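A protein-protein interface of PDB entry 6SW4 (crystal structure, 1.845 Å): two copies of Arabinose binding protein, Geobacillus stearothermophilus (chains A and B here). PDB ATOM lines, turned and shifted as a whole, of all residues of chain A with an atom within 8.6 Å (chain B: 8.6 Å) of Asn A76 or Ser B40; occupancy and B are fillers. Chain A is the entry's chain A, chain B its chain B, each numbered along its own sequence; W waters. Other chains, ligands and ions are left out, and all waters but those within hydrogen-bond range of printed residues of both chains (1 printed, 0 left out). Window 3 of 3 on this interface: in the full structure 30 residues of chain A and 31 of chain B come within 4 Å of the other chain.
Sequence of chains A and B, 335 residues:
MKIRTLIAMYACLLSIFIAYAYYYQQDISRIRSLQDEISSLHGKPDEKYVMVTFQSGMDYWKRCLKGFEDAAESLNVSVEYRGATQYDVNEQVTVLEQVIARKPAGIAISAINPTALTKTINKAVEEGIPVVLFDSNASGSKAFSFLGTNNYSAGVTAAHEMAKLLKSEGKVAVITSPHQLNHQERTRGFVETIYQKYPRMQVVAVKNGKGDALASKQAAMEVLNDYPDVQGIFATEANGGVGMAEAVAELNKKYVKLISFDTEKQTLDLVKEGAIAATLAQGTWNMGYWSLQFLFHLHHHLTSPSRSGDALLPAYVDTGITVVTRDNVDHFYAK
Asn A76 touches just these residues of chain B: Ile B38 (2.8 Å), Ser B39 (3.7 Å) and Ser B40 (2.8 Å). Of chain A, only Ser A74 and Asn A76 come within 4 Å of Ser B40. No residue of chain B comes within 4 Å of Val A77. Of chain A, only Ser A74 (3.8 Å), Leu A75 (3.4 Å) and Asn A76 (3.7 Å) come within 4 Å of Ser B39. Of the printed residues of chain B, Leu A75 touches Ile B38 and Ser B39. Of the printed residues of chain B, Ser A74 touches Ser B39 (3.8 Å), Ser B40 (2.8 Å) and Leu B41 (2.9 Å). Of the printed residues of chain B, Gln A293 touches Leu B41. Leu B302 touches none of the printed residues of chain A. Ala A71 touches none of the printed residues of chain B. The nearest residue of chain B that does not touch Asn A76 is Leu B41 (6.1 Å).
O of Ser A74 touches OG of Ser B39 (3.8 Å). OG of Ser A74 touches CD2 of Leu B41 (2.9 Å). O of Ile B38 touches O of Leu A75, 3.7 Å away. Leu A75 touches Ser B39. Ser B39 touches Asn A76. Gln A293 touches Leu B41.
Water W1 lies within hydrogen-bond range of the backbone carbonyl oxygen (O) of Glu A73 (2.6 Å), the side-chain amide oxygen (OD1) of Asn A76 (2.6 Å) and the side-chain hydroxyl (OG) of Ser B40 (2.8 Å).
Positions printed for both chains: 74, 75, 296 and 300.
Of the 20 printed residues of chain A, 4 touch a printed residue of chain B. Hydrophobic or aromatic side chains of chain B within 4 Å of the printed part of chain A: Leu B41. Along chain B the printed residues that touch a printed residue of chain A span positions 38 to 41. Among the printed residues, 9 pairs touch across the chains. Among the printed residues, no Asp or Glu carboxylate lies within 4 Å of a Lys or Arg side-chain nitrogen of the other chain.
The side-chain hydroxyl (OG) of Ser B39 lies within hydrogen-bond range of the backbone NH (N) of Leu B41 (2.8 Å). The backbone carbonyl oxygen (O) of Ser B39 lies close to a ring nitrogen (ND1) of His B42 (3.1 Å).
N of Ser B40 is in hydrogen-bond range of O of Ser A74 (2.8 Å). The side-chain amide nitrogen of Asn A76 is in hydrogen-bond range of the backbone carbonyl oxygen of Ile B38 (2.8 Å). The side-chain hydroxyl (OG) of Ser B40 lies within hydrogen-bond range of the side-chain amide nitrogen (ND2) of Asn A76, 2.8 Å away.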
ATOM      1  N   ASP A  46      -4.374  -6.910   2.519  1.00  0.00           N
ATOM      2  CA  ASP A  46      -4.084  -8.339   2.575  1.00  0.00           C
ATOM      3  C   ASP A  46      -2.849  -8.581   3.439  1.00  0.00           C
ATOM      4  O   ASP A  46      -1.767  -8.054   3.154  1.00  0.00           O
ATOM      5  CB  ASP A  46      -3.882  -8.907   1.170  1.00  0.00           C
ATOM      6  CG  ASP A  46      -3.093 -10.210   1.171  1.00  0.00           C
ATOM      7  OD1 ASP A  46      -3.630 -11.242   1.635  1.00  0.00           O
ATOM      8  OD2 ASP A  46      -1.932 -10.200   0.703  1.00  0.00           O
ATOM      9  N   GLU A  47      -3.015  -9.400   4.475  1.00  0.00           N
ATOM     10  CA  GLU A  47      -2.001  -9.661   5.499  1.00  0.00           C
ATOM     11  C   GLU A  47      -0.979 -10.671   4.972  1.00  0.00           C
ATOM     12  O   GLU A  47      -1.205 -11.884   5.014  1.00  0.00           O
ATOM     13  CB  GLU A  47      -2.700 -10.164   6.758  1.00  0.00           C
ATOM     14  CG  GLU A  47      -1.847 -10.370   7.980  1.00  0.00           C
ATOM     15  CD  GLU A  47      -2.712 -10.645   9.196  1.00  0.00           C
ATOM     16  OE1 GLU A  47      -3.947 -10.573   9.066  1.00  0.00           O
ATOM     17  OE2 GLU A  47      -2.175 -10.950  10.270  1.00  0.00           O
ATOM     18  N   LYS A  48       0.164 -10.175   4.493  1.00  0.00           N
ATOM     19  CA  LYS A  48       1.183 -10.992   3.844  1.00  0.00           C
ATOM     20  C   LYS A  48       2.493 -10.915   4.624  1.00  0.00           C
ATOM     21  O   LYS A  48       2.935  -9.820   4.997  1.00  0.00           O
ATOM     22  CB  LYS A  48       1.401 -10.540   2.391  1.00  0.00           C
ATOM     23  CG  LYS A  48       2.077 -11.591   1.487  1.00  0.00           C
ATOM     24  CD  LYS A  48       2.014 -11.223  -0.001  1.00  0.00           C
ATOM     25  CE  LYS A  48       3.009 -10.120  -0.331  1.00  0.00           C
ATOM     26  NZ  LYS A  48       3.039  -9.760  -1.780  1.00  0.00           N
ATOM     27  N   TYR A  49       3.114 -12.074   4.860  1.00  0.00           N
ATOM     28  CA  TYR A  49       4.392 -12.174   5.560  1.00  0.00           C
ATOM     29  C   TYR A  49       5.446 -12.707   4.599  1.00  0.00           C
ATOM     30  O   TYR A  49       5.188 -13.656   3.855  1.00  0.00           O
ATOM     31  CB  TYR A  49       4.273 -13.080   6.780  1.00  0.00           C
ATOM     32  CG  TYR A  49       3.323 -12.527   7.809  1.00  0.00           C
ATOM     33  CD1 TYR A  49       1.944 -12.724   7.697  1.00  0.00           C
ATOM     34  CD2 TYR A  49       3.797 -11.765   8.872  1.00  0.00           C
ATOM     35  CE1 TYR A  49       1.064 -12.201   8.649  1.00  0.00           C
ATOM     36  CE2 TYR A  49       2.930 -11.241   9.829  1.00  0.00           C
ATOM     37  CZ  TYR A  49       1.566 -11.453   9.711  1.00  0.00           C
ATOM     38  OH  TYR A  49       0.721 -10.914  10.662  1.00  0.00           O
ATOM     39  N   PHE A  68       6.918 -21.930   7.309  1.00  0.00           N
ATOM     40  CA  PHE A  68       6.248 -20.642   7.131  1.00  0.00           C
ATOM     41  C   PHE A  68       4.843 -20.831   6.547  1.00  0.00           C
ATOM     42  O   PHE A  68       3.853 -20.329   7.093  1.00  0.00           O
ATOM     43  CB  PHE A  68       7.103 -19.789   6.190  1.00  0.00           C
ATOM     44  CG  PHE A  68       7.137 -18.315   6.516  1.00  0.00           C
ATOM     45  CD1 PHE A  68       7.419 -17.868   7.794  1.00  0.00           C
ATOM     46  CD2 PHE A  68       6.949 -17.378   5.506  1.00  0.00           C
ATOM     47  CE1 PHE A  68       7.484 -16.525   8.074  1.00  0.00           C
ATOM     48  CE2 PHE A  68       7.006 -16.019   5.784  1.00  0.00           C
ATOM     49  CZ  PHE A  68       7.266 -15.597   7.076  1.00  0.00           C
ATOM     50  N   GLU A  69       4.743 -21.572   5.436  1.00  0.00           N
ATOM     51  CA  GLU A  69       3.438 -21.793   4.796  1.00  0.00           C
ATOM     52  C   GLU A  69       2.492 -22.575   5.695  1.00  0.00           C
ATOM     53  O   GLU A  69       1.292 -22.293   5.729  1.00  0.00           O
ATOM     54  CB  GLU A  69       3.614 -22.525   3.466  1.00  0.00           C
ATOM     55  CG  GLU A  69       4.379 -21.708   2.446  1.00  0.00           C
ATOM     56  CD  GLU A  69       4.604 -22.459   1.148  1.00  0.00           C
ATOM     57  OE1 GLU A  69       4.324 -23.677   1.108  1.00  0.00           O
ATOM     58  OE2 GLU A  69       5.070 -21.832   0.169  1.00  0.00           O
ATOM     59  N   ASP A  70       3.005 -23.574   6.414  1.00  0.00           N
ATOM     60  CA  ASP A  70       2.174 -24.324   7.352  1.00  0.00           C
ATOM     61  C   ASP A  70       1.621 -23.430   8.450  1.00  0.00           C
ATOM     62  O   ASP A  70       0.471 -23.595   8.877  1.00  0.00           O
ATOM     63  CB  ASP A  70       2.977 -25.457   7.974  1.00  0.00           C
ATOM     64  CG  ASP A  70       3.056 -26.679   7.080  1.00  0.00           C
ATOM     65  OD1 ASP A  70       2.486 -26.669   5.955  1.00  0.00           O
ATOM     66  OD2 ASP A  70       3.685 -27.655   7.523  1.00  0.00           O
ATOM     67  N   ALA A  71       2.438 -22.510   8.964  1.00  0.00           N
ATOM     68  CA  ALA A  71       1.930 -21.547   9.937  1.00  0.00           C
ATOM     69  C   ALA A  71       0.902 -20.622   9.306  1.00  0.00           C
ATOM     70  O   ALA A  71      -0.119 -20.309   9.930  1.00  0.00           O
ATOM     71  CB  ALA A  71       3.071 -20.720  10.538  1.00  0.00           C
ATOM     72  N   ALA A  72       1.153 -20.174   8.068  1.00  0.00           N
ATOM     73  CA  ALA A  72       0.221 -19.274   7.386  1.00  0.00           C
ATOM     74  C   ALA A  72      -1.112 -19.953   7.100  1.00  0.00           C
ATOM     75  O   ALA A  72      -2.161 -19.301   7.125  1.00  0.00           O
ATOM     76  CB  ALA A  72       0.823 -18.777   6.070  1.00  0.00           C
ATOM     77  N   GLU A  73      -1.086 -21.248   6.783  1.00  0.00           N
ATOM     78  CA  GLU A  73      -2.324 -21.964   6.490  1.00  0.00           C
ATOM     79  C   GLU A  73      -3.133 -22.211   7.749  1.00  0.00           C
ATOM     80  O   GLU A  73      -4.355 -22.384   7.684  1.00  0.00           O
ATOM     81  CB  GLU A  73      -2.005 -23.276   5.784  1.00  0.00           C
ATOM     82  CG  GLU A  73      -1.492 -23.026   4.367  1.00  0.00           C
ATOM     83  CD  GLU A  73      -0.799 -24.228   3.747  1.00  0.00           C
ATOM     84  OE1 GLU A  73      -0.986 -25.363   4.245  1.00  0.00           O
ATOM     85  OE2 GLU A  73      -0.085 -24.027   2.734  1.00  0.00           O
ATOM     86  N   SER A  74      -2.470 -22.220   8.896  1.00  0.00           N
ATOM     87  CA  SER A  74      -3.183 -22.265  10.159  1.00  0.00           C
ATOM     88  C   SER A  74      -3.595 -20.876  10.622  1.00  0.00           C
ATOM     89  O   SER A  74      -4.568 -20.742  11.374  1.00  0.00           O
ATOM     90  CB  SER A  74      -2.311 -22.929  11.213  1.00  0.00           C
ATOM     91  OG  SER A  74      -3.016 -22.910  12.440  1.00  0.00           O
ATOM     92  N   LEU A  75      -2.868 -19.838  10.200  1.00  0.00           N
ATOM     93  CA  LEU A  75      -3.231 -18.479  10.571  1.00  0.00           C
ATOM     94  C   LEU A  75      -4.121 -17.808   9.541  1.00  0.00           C
ATOM     95  O   LEU A  75      -4.620 -16.712   9.805  1.00  0.00           O
ATOM     96  CB  LEU A  75      -1.983 -17.616  10.783  1.00  0.00           C
ATOM     97  CG  LEU A  75      -1.119 -18.082  11.955  1.00  0.00           C
ATOM     98  CD1 LEU A  75       0.279 -17.454  11.857  1.00  0.00           C
ATOM     99  CD2 LEU A  75      -1.792 -17.770  13.294  1.00  0.00           C
ATOM    100  N   ASN A  76      -4.321 -18.432   8.384  1.00  0.00           N
ATOM    101  CA  ASN A  76      -5.090 -17.821   7.312  1.00  0.00           C
ATOM    102  C   ASN A  76      -4.491 -16.465   6.934  1.00  0.00           C
ATOM    103  O   ASN A  76      -5.197 -15.461   6.804  1.00  0.00           O
ATOM    104  CB  ASN A  76      -6.567 -17.703   7.711  1.00  0.00           C
ATOM    105  CG  ASN A  76      -7.177 -19.050   8.065  1.00  0.00           C
ATOM    106  OD1 ASN A  76      -6.999 -20.032   7.332  1.00  0.00           O
ATOM    107  ND2 ASN A  76      -7.878 -19.116   9.193  1.00  0.00           N
ATOM    108  N   VAL A  77      -3.158 -16.434   6.787  1.00  0.00           N
ATOM    109  CA  VAL A  77      -2.507 -15.263   6.227  1.00  0.00           C
ATOM    110  C   VAL A  77      -1.711 -15.707   5.012  1.00  0.00           C
ATOM    111  O   VAL A  77      -1.532 -16.899   4.758  1.00  0.00           O
ATOM    112  CB  VAL A  77      -1.621 -14.508   7.240  1.00  0.00           C
ATOM    113  CG1 VAL A  77      -2.442 -14.071   8.453  1.00  0.00           C
ATOM    114  CG2 VAL A  77      -0.432 -15.365   7.664  1.00  0.00           C
ATOM    115  N   SER A  78      -1.311 -14.724   4.217  1.00  0.00           N
ATOM    116  CA  SER A  78      -0.507 -14.910   3.022  1.00  0.00           C
ATOM    117  C   SER A  78       0.965 -15.000   3.410  1.00  0.00           C
ATOM    118  O   SER A  78       1.381 -14.447   4.427  1.00  0.00           O
ATOM    119  CB  SER A  78      -0.710 -13.737   2.055  1.00  0.00           C
ATOM    120  OG  SER A  78      -1.788 -13.968   1.170  1.00  0.00           O
ATOM    121  N   VAL A  79       1.760 -15.698   2.585  1.00  0.00           N
ATOM    122  CA  VAL A  79       3.213 -15.610   2.695  1.00  0.00           C
ATOM    123  C   VAL A  79       3.820 -15.501   1.305  1.00  0.00           C
ATOM    124  O   VAL A  79       3.209 -15.875   0.302  1.00  0.00           O
ATOM    125  CB  VAL A  79       3.856 -16.792   3.473  1.00  0.00           C
ATOM    126  CG1 VAL A  79       3.402 -16.785   4.938  1.00  0.00           C
ATOM    127  CG2 VAL A  79       3.557 -18.126   2.817  1.00  0.00           C
ATOM    128  N   LEU A 292       6.788 -17.241  11.672  1.00  0.00           N
ATOM    129  CA  LEU A 292       5.502 -16.647  11.317  1.00  0.00           C
ATOM    130  C   LEU A 292       4.641 -16.443  12.550  1.00  0.00           C
ATOM    131  O   LEU A 292       3.990 -15.404  12.676  1.00  0.00           O
ATOM    132  CB  LEU A 292       4.762 -17.501  10.291  1.00  0.00           C
ATOM    133  CG  LEU A 292       3.853 -16.700   9.329  1.00  0.00           C
ATOM    134  CD1 LEU A 292       3.215 -17.602   8.323  1.00  0.00           C
ATOM    135  CD2 LEU A 292       2.791 -15.978  10.025  1.00  0.00           C
ATOM    136  N   GLN A 293       4.622 -17.417  13.462  1.00  0.00           N
ATOM    137  CA  GLN A 293       3.864 -17.288  14.700  1.00  0.00           C
ATOM    138  C   GLN A 293       4.270 -16.042  15.473  1.00  0.00           C
ATOM    139  O   GLN A 293       3.424 -15.284  15.974  1.00  0.00           O
ATOM    140  CB  GLN A 293       4.057 -18.527  15.566  1.00  0.00           C
ATOM    141  CG  GLN A 293       3.402 -19.767  15.017  1.00  0.00           C
ATOM    142  CD  GLN A 293       1.899 -19.764  15.264  1.00  0.00           C
ATOM    143  OE1 GLN A 293       1.385 -20.491  16.124  1.00  0.00           O
ATOM    144  NE2 GLN A 293       1.199 -18.928  14.540  1.00  0.00           N
ATOM    145  N   PHE A 296       3.241 -12.890  13.158  1.00  0.00           N
ATOM    146  CA  PHE A 296       1.800 -12.695  13.266  1.00  0.00           C
ATOM    147  C   PHE A 296       1.459 -12.078  14.607  1.00  0.00           C
ATOM    148  O   PHE A 296       0.619 -11.175  14.699  1.00  0.00           O
ATOM    149  CB  PHE A 296       1.083 -14.036  13.083  1.00  0.00           C
ATOM    150  CG  PHE A 296      -0.399 -13.995  13.371  1.00  0.00           C
ATOM    151  CD1 PHE A 296      -0.878 -14.175  14.666  1.00  0.00           C
ATOM    152  CD2 PHE A 296      -1.314 -13.823  12.339  1.00  0.00           C
ATOM    153  CE1 PHE A 296      -2.233 -14.151  14.926  1.00  0.00           C
ATOM    154  CE2 PHE A 296      -2.672 -13.808  12.603  1.00  0.00           C
ATOM    155  CZ  PHE A 296      -3.119 -13.969  13.908  1.00  0.00           C
ATOM    156  N   HIS A 300      -0.225  -8.020  15.677  1.00  0.00           N
ATOM    157  CA  HIS A 300      -1.487  -7.868  16.389  1.00  0.00           C
ATOM    158  C   HIS A 300      -1.296  -7.353  17.808  1.00  0.00           C
ATOM    159  O   HIS A 300      -2.218  -7.478  18.625  1.00  0.00           O
ATOM    160  CB  HIS A 300      -2.246  -9.196  16.437  1.00  0.00           C
ATOM    161  CG  HIS A 300      -2.586  -9.759  15.094  1.00  0.00           C
ATOM    162  ND1 HIS A 300      -3.714 -10.517  14.877  1.00  0.00           N
ATOM    163  CD2 HIS A 300      -1.939  -9.698  13.905  1.00  0.00           C
ATOM    164  CE1 HIS A 300      -3.754 -10.889  13.609  1.00  0.00           C
ATOM    165  NE2 HIS A 300      -2.688 -10.407  12.998  1.00  0.00           N
ATOM    166  N   ILE B  38      -8.822 -13.900  10.029  1.00  0.00           N
ATOM    167  CA  ILE B  38      -8.900 -14.546  11.373  1.00  0.00           C
ATOM    168  C   ILE B  38      -8.153 -15.881  11.323  1.00  0.00           C
ATOM    169  O   ILE B  38      -8.276 -16.598  10.313  1.00  0.00           O
ATOM    170  CB  ILE B  38     -10.363 -14.724  11.821  1.00  0.00           C
ATOM    171  CG1 ILE B  38     -11.146 -13.413  11.740  1.00  0.00           C
ATOM    172  CG2 ILE B  38     -10.432 -15.329  13.215  1.00  0.00           C
ATOM    173  CD1 ILE B  38     -12.392 -13.398  12.594  1.00  0.00           C
ATOM    174  N   SER B  39      -7.413 -16.191  12.388  1.00  0.00           N
ATOM    175  CA  SER B  39      -6.578 -17.417  12.448  1.00  0.00           C
ATOM    176  C   SER B  39      -7.453 -18.620  12.818  1.00  0.00           C
ATOM    177  O   SER B  39      -8.546 -18.410  13.363  1.00  0.00           O
ATOM    178  CB  SER B  39      -5.443 -17.221  13.421  1.00  0.00           C
ATOM    179  OG  SER B  39      -5.252 -18.358  14.241  1.00  0.00           O
ATOM    180  N   SER B  40      -6.980 -19.827  12.507  1.00  0.00           N
ATOM    181  CA  SER B  40      -7.711 -21.073  12.846  1.00  0.00           C
ATOM    182  C   SER B  40      -7.113 -21.669  14.125  1.00  0.00           C
ATOM    183  O   SER B  40      -7.469 -22.812  14.452  1.00  0.00           O
ATOM    184  CB  SER B  40      -7.643 -22.060  11.712  1.00  0.00           C
ATOM    185  OG  SER B  40      -8.246 -21.535  10.545  1.00  0.00           O
ATOM    186  N   LEU B  41      -6.248 -20.912  14.815  1.00  0.00           N
ATOM    187  CA  LEU B  41      -5.594 -21.422  16.018  1.00  0.00           C
ATOM    188  C   LEU B  41      -6.454 -21.199  17.253  1.00  0.00           C
ATOM    189  O   LEU B  41      -6.002 -20.591  18.229  1.00  0.00           O
ATOM    190  CB  LEU B  41      -4.221 -20.763  16.210  1.00  0.00           C
ATOM    191  CG  LEU B  41      -3.073 -21.364  15.402  1.00  0.00           C
ATOM    192  CD1 LEU B  41      -1.722 -21.017  16.041  1.00  0.00           C
ATOM    193  CD2 LEU B  41      -3.246 -22.868  15.358  1.00  0.00           C
ATOM    194  N   HIS B  42      -7.684 -21.700  17.235  1.00  0.00           N
ATOM    195  CA  HIS B  42      -8.610 -21.528  18.346  1.00  0.00           C
ATOM    196  C   HIS B  42      -9.075 -22.880  18.862  1.00  0.00           C
ATOM    197  O   HIS B  42      -9.437 -23.758  18.076  1.00  0.00           O
ATOM    198  CB  HIS B  42      -9.812 -20.685  17.926  1.00  0.00           C
ATOM    199  CG  HIS B  42      -9.461 -19.284  17.551  1.00  0.00           C
ATOM    200  ND1 HIS B  42      -9.492 -18.831  16.250  1.00  0.00           N
ATOM    201  CD2 HIS B  42      -9.047 -18.237  18.306  1.00  0.00           C
ATOM    202  CE1 HIS B  42      -9.132 -17.560  16.220  1.00  0.00           C
ATOM    203  NE2 HIS B  42      -8.856 -17.176  17.454  1.00  0.00           N
ATOM    204  N   GLY B  43      -9.261 -22.903  20.166  1.00  0.00           N
ATOM    205  CA  GLY B  43      -9.878 -24.076  20.771  1.00  0.00           C
ATOM    206  C   GLY B  43     -11.155 -23.655  21.454  1.00  0.00           C
ATOM    207  O   GLY B  43     -11.748 -22.662  21.016  1.00  0.00           O
ATOM    208  N   SER B  74      -6.539 -15.700  23.737  1.00  0.00           N
ATOM    209  CA  SER B  74      -6.324 -15.695  22.298  1.00  0.00           C
ATOM    210  C   SER B  74      -6.619 -17.059  21.681  1.00  0.00           C
ATOM    211  O   SER B  74      -6.984 -17.134  20.503  1.00  0.00           O
ATOM    212  CB  SER B  74      -4.880 -15.260  21.992  1.00  0.00           C
ATOM    213  OG  SER B  74      -4.625 -15.181  20.595  1.00  0.00           O
ATOM    214  N   LEU B  75      -6.475 -18.123  22.473  1.00  0.00           N
ATOM    215  CA  LEU B  75      -6.688 -19.504  21.965  1.00  0.00           C
ATOM    216  C   LEU B  75      -8.116 -19.975  22.259  1.00  0.00           C
ATOM    217  O   LEU B  75      -8.459 -21.087  21.821  1.00  0.00           O
ATOM    218  CB  LEU B  75      -5.681 -20.429  22.651  1.00  0.00           C
ATOM    219  CG  LEU B  75      -4.220 -20.207  22.274  1.00  0.00           C
ATOM    220  CD1 LEU B  75      -3.301 -20.943  23.231  1.00  0.00           C
ATOM    221  CD2 LEU B  75      -3.965 -20.645  20.842  1.00  0.00           C
ATOM    222  N   PHE B 296      -0.604 -25.730  23.665  1.00  0.00           N
ATOM    223  CA  PHE B 296      -1.689 -25.801  22.690  1.00  0.00           C
ATOM    224  C   PHE B 296      -1.229 -26.511  21.426  1.00  0.00           C
ATOM    225  O   PHE B 296      -1.939 -27.369  20.889  1.00  0.00           O
ATOM    226  CB  PHE B 296      -2.205 -24.407  22.369  1.00  0.00           C
ATOM    227  CG  PHE B 296      -3.395 -24.398  21.449  1.00  0.00           C
ATOM    228  CD1 PHE B 296      -3.227 -24.428  20.070  1.00  0.00           C
ATOM    229  CD2 PHE B 296      -4.684 -24.360  21.963  1.00  0.00           C
ATOM    230  CE1 PHE B 296      -4.329 -24.419  19.226  1.00  0.00           C
ATOM    231  CE2 PHE B 296      -5.775 -24.332  21.136  1.00  0.00           C
ATOM    232  CZ  PHE B 296      -5.607 -24.368  19.767  1.00  0.00           C
ATOM    233  N   HIS B 300      -2.811 -30.260  20.355  1.00  0.00           N
ATOM    234  CA  HIS B 300      -3.458 -30.405  19.060  1.00  0.00           C
ATOM    235  C   HIS B 300      -2.528 -30.964  17.987  1.00  0.00           C
ATOM    236  O   HIS B 300      -2.898 -30.957  16.804  1.00  0.00           O
ATOM    237  CB  HIS B 300      -4.032 -29.059  18.620  1.00  0.00           C
ATOM    238  CG  HIS B 300      -5.119 -28.563  19.514  1.00  0.00           C
ATOM    239  ND1 HIS B 300      -6.418 -29.019  19.422  1.00  0.00           N
ATOM    240  CD2 HIS B 300      -5.103 -27.675  20.537  1.00  0.00           C
ATOM    241  CE1 HIS B 300      -7.156 -28.426  20.345  1.00  0.00           C
ATOM    242  NE2 HIS B 300      -6.383 -27.609  21.037  1.00  0.00           N
ATOM    243  N   LEU B 302       0.118 -30.047  16.357  1.00  0.00           N
ATOM    244  CA  LEU B 302       0.294 -29.119  15.250  1.00  0.00           C
ATOM    245  C   LEU B 302       1.727 -29.065  14.744  1.00  0.00           C
ATOM    246  O   LEU B 302       2.006 -28.343  13.779  1.00  0.00           O
ATOM    247  CB  LEU B 302      -0.154 -27.721  15.667  1.00  0.00           C
ATOM    248  CG  LEU B 302      -1.643 -27.586  15.974  1.00  0.00           C
ATOM    249  CD1 LEU B 302      -1.921 -26.192  16.499  1.00  0.00           C
ATOM    250  CD2 LEU B 302      -2.467 -27.862  14.711  1.00  0.00           C
HETATM  251  O   HOH W   1      -6.852 -22.443   8.301  1.00  0.00           O
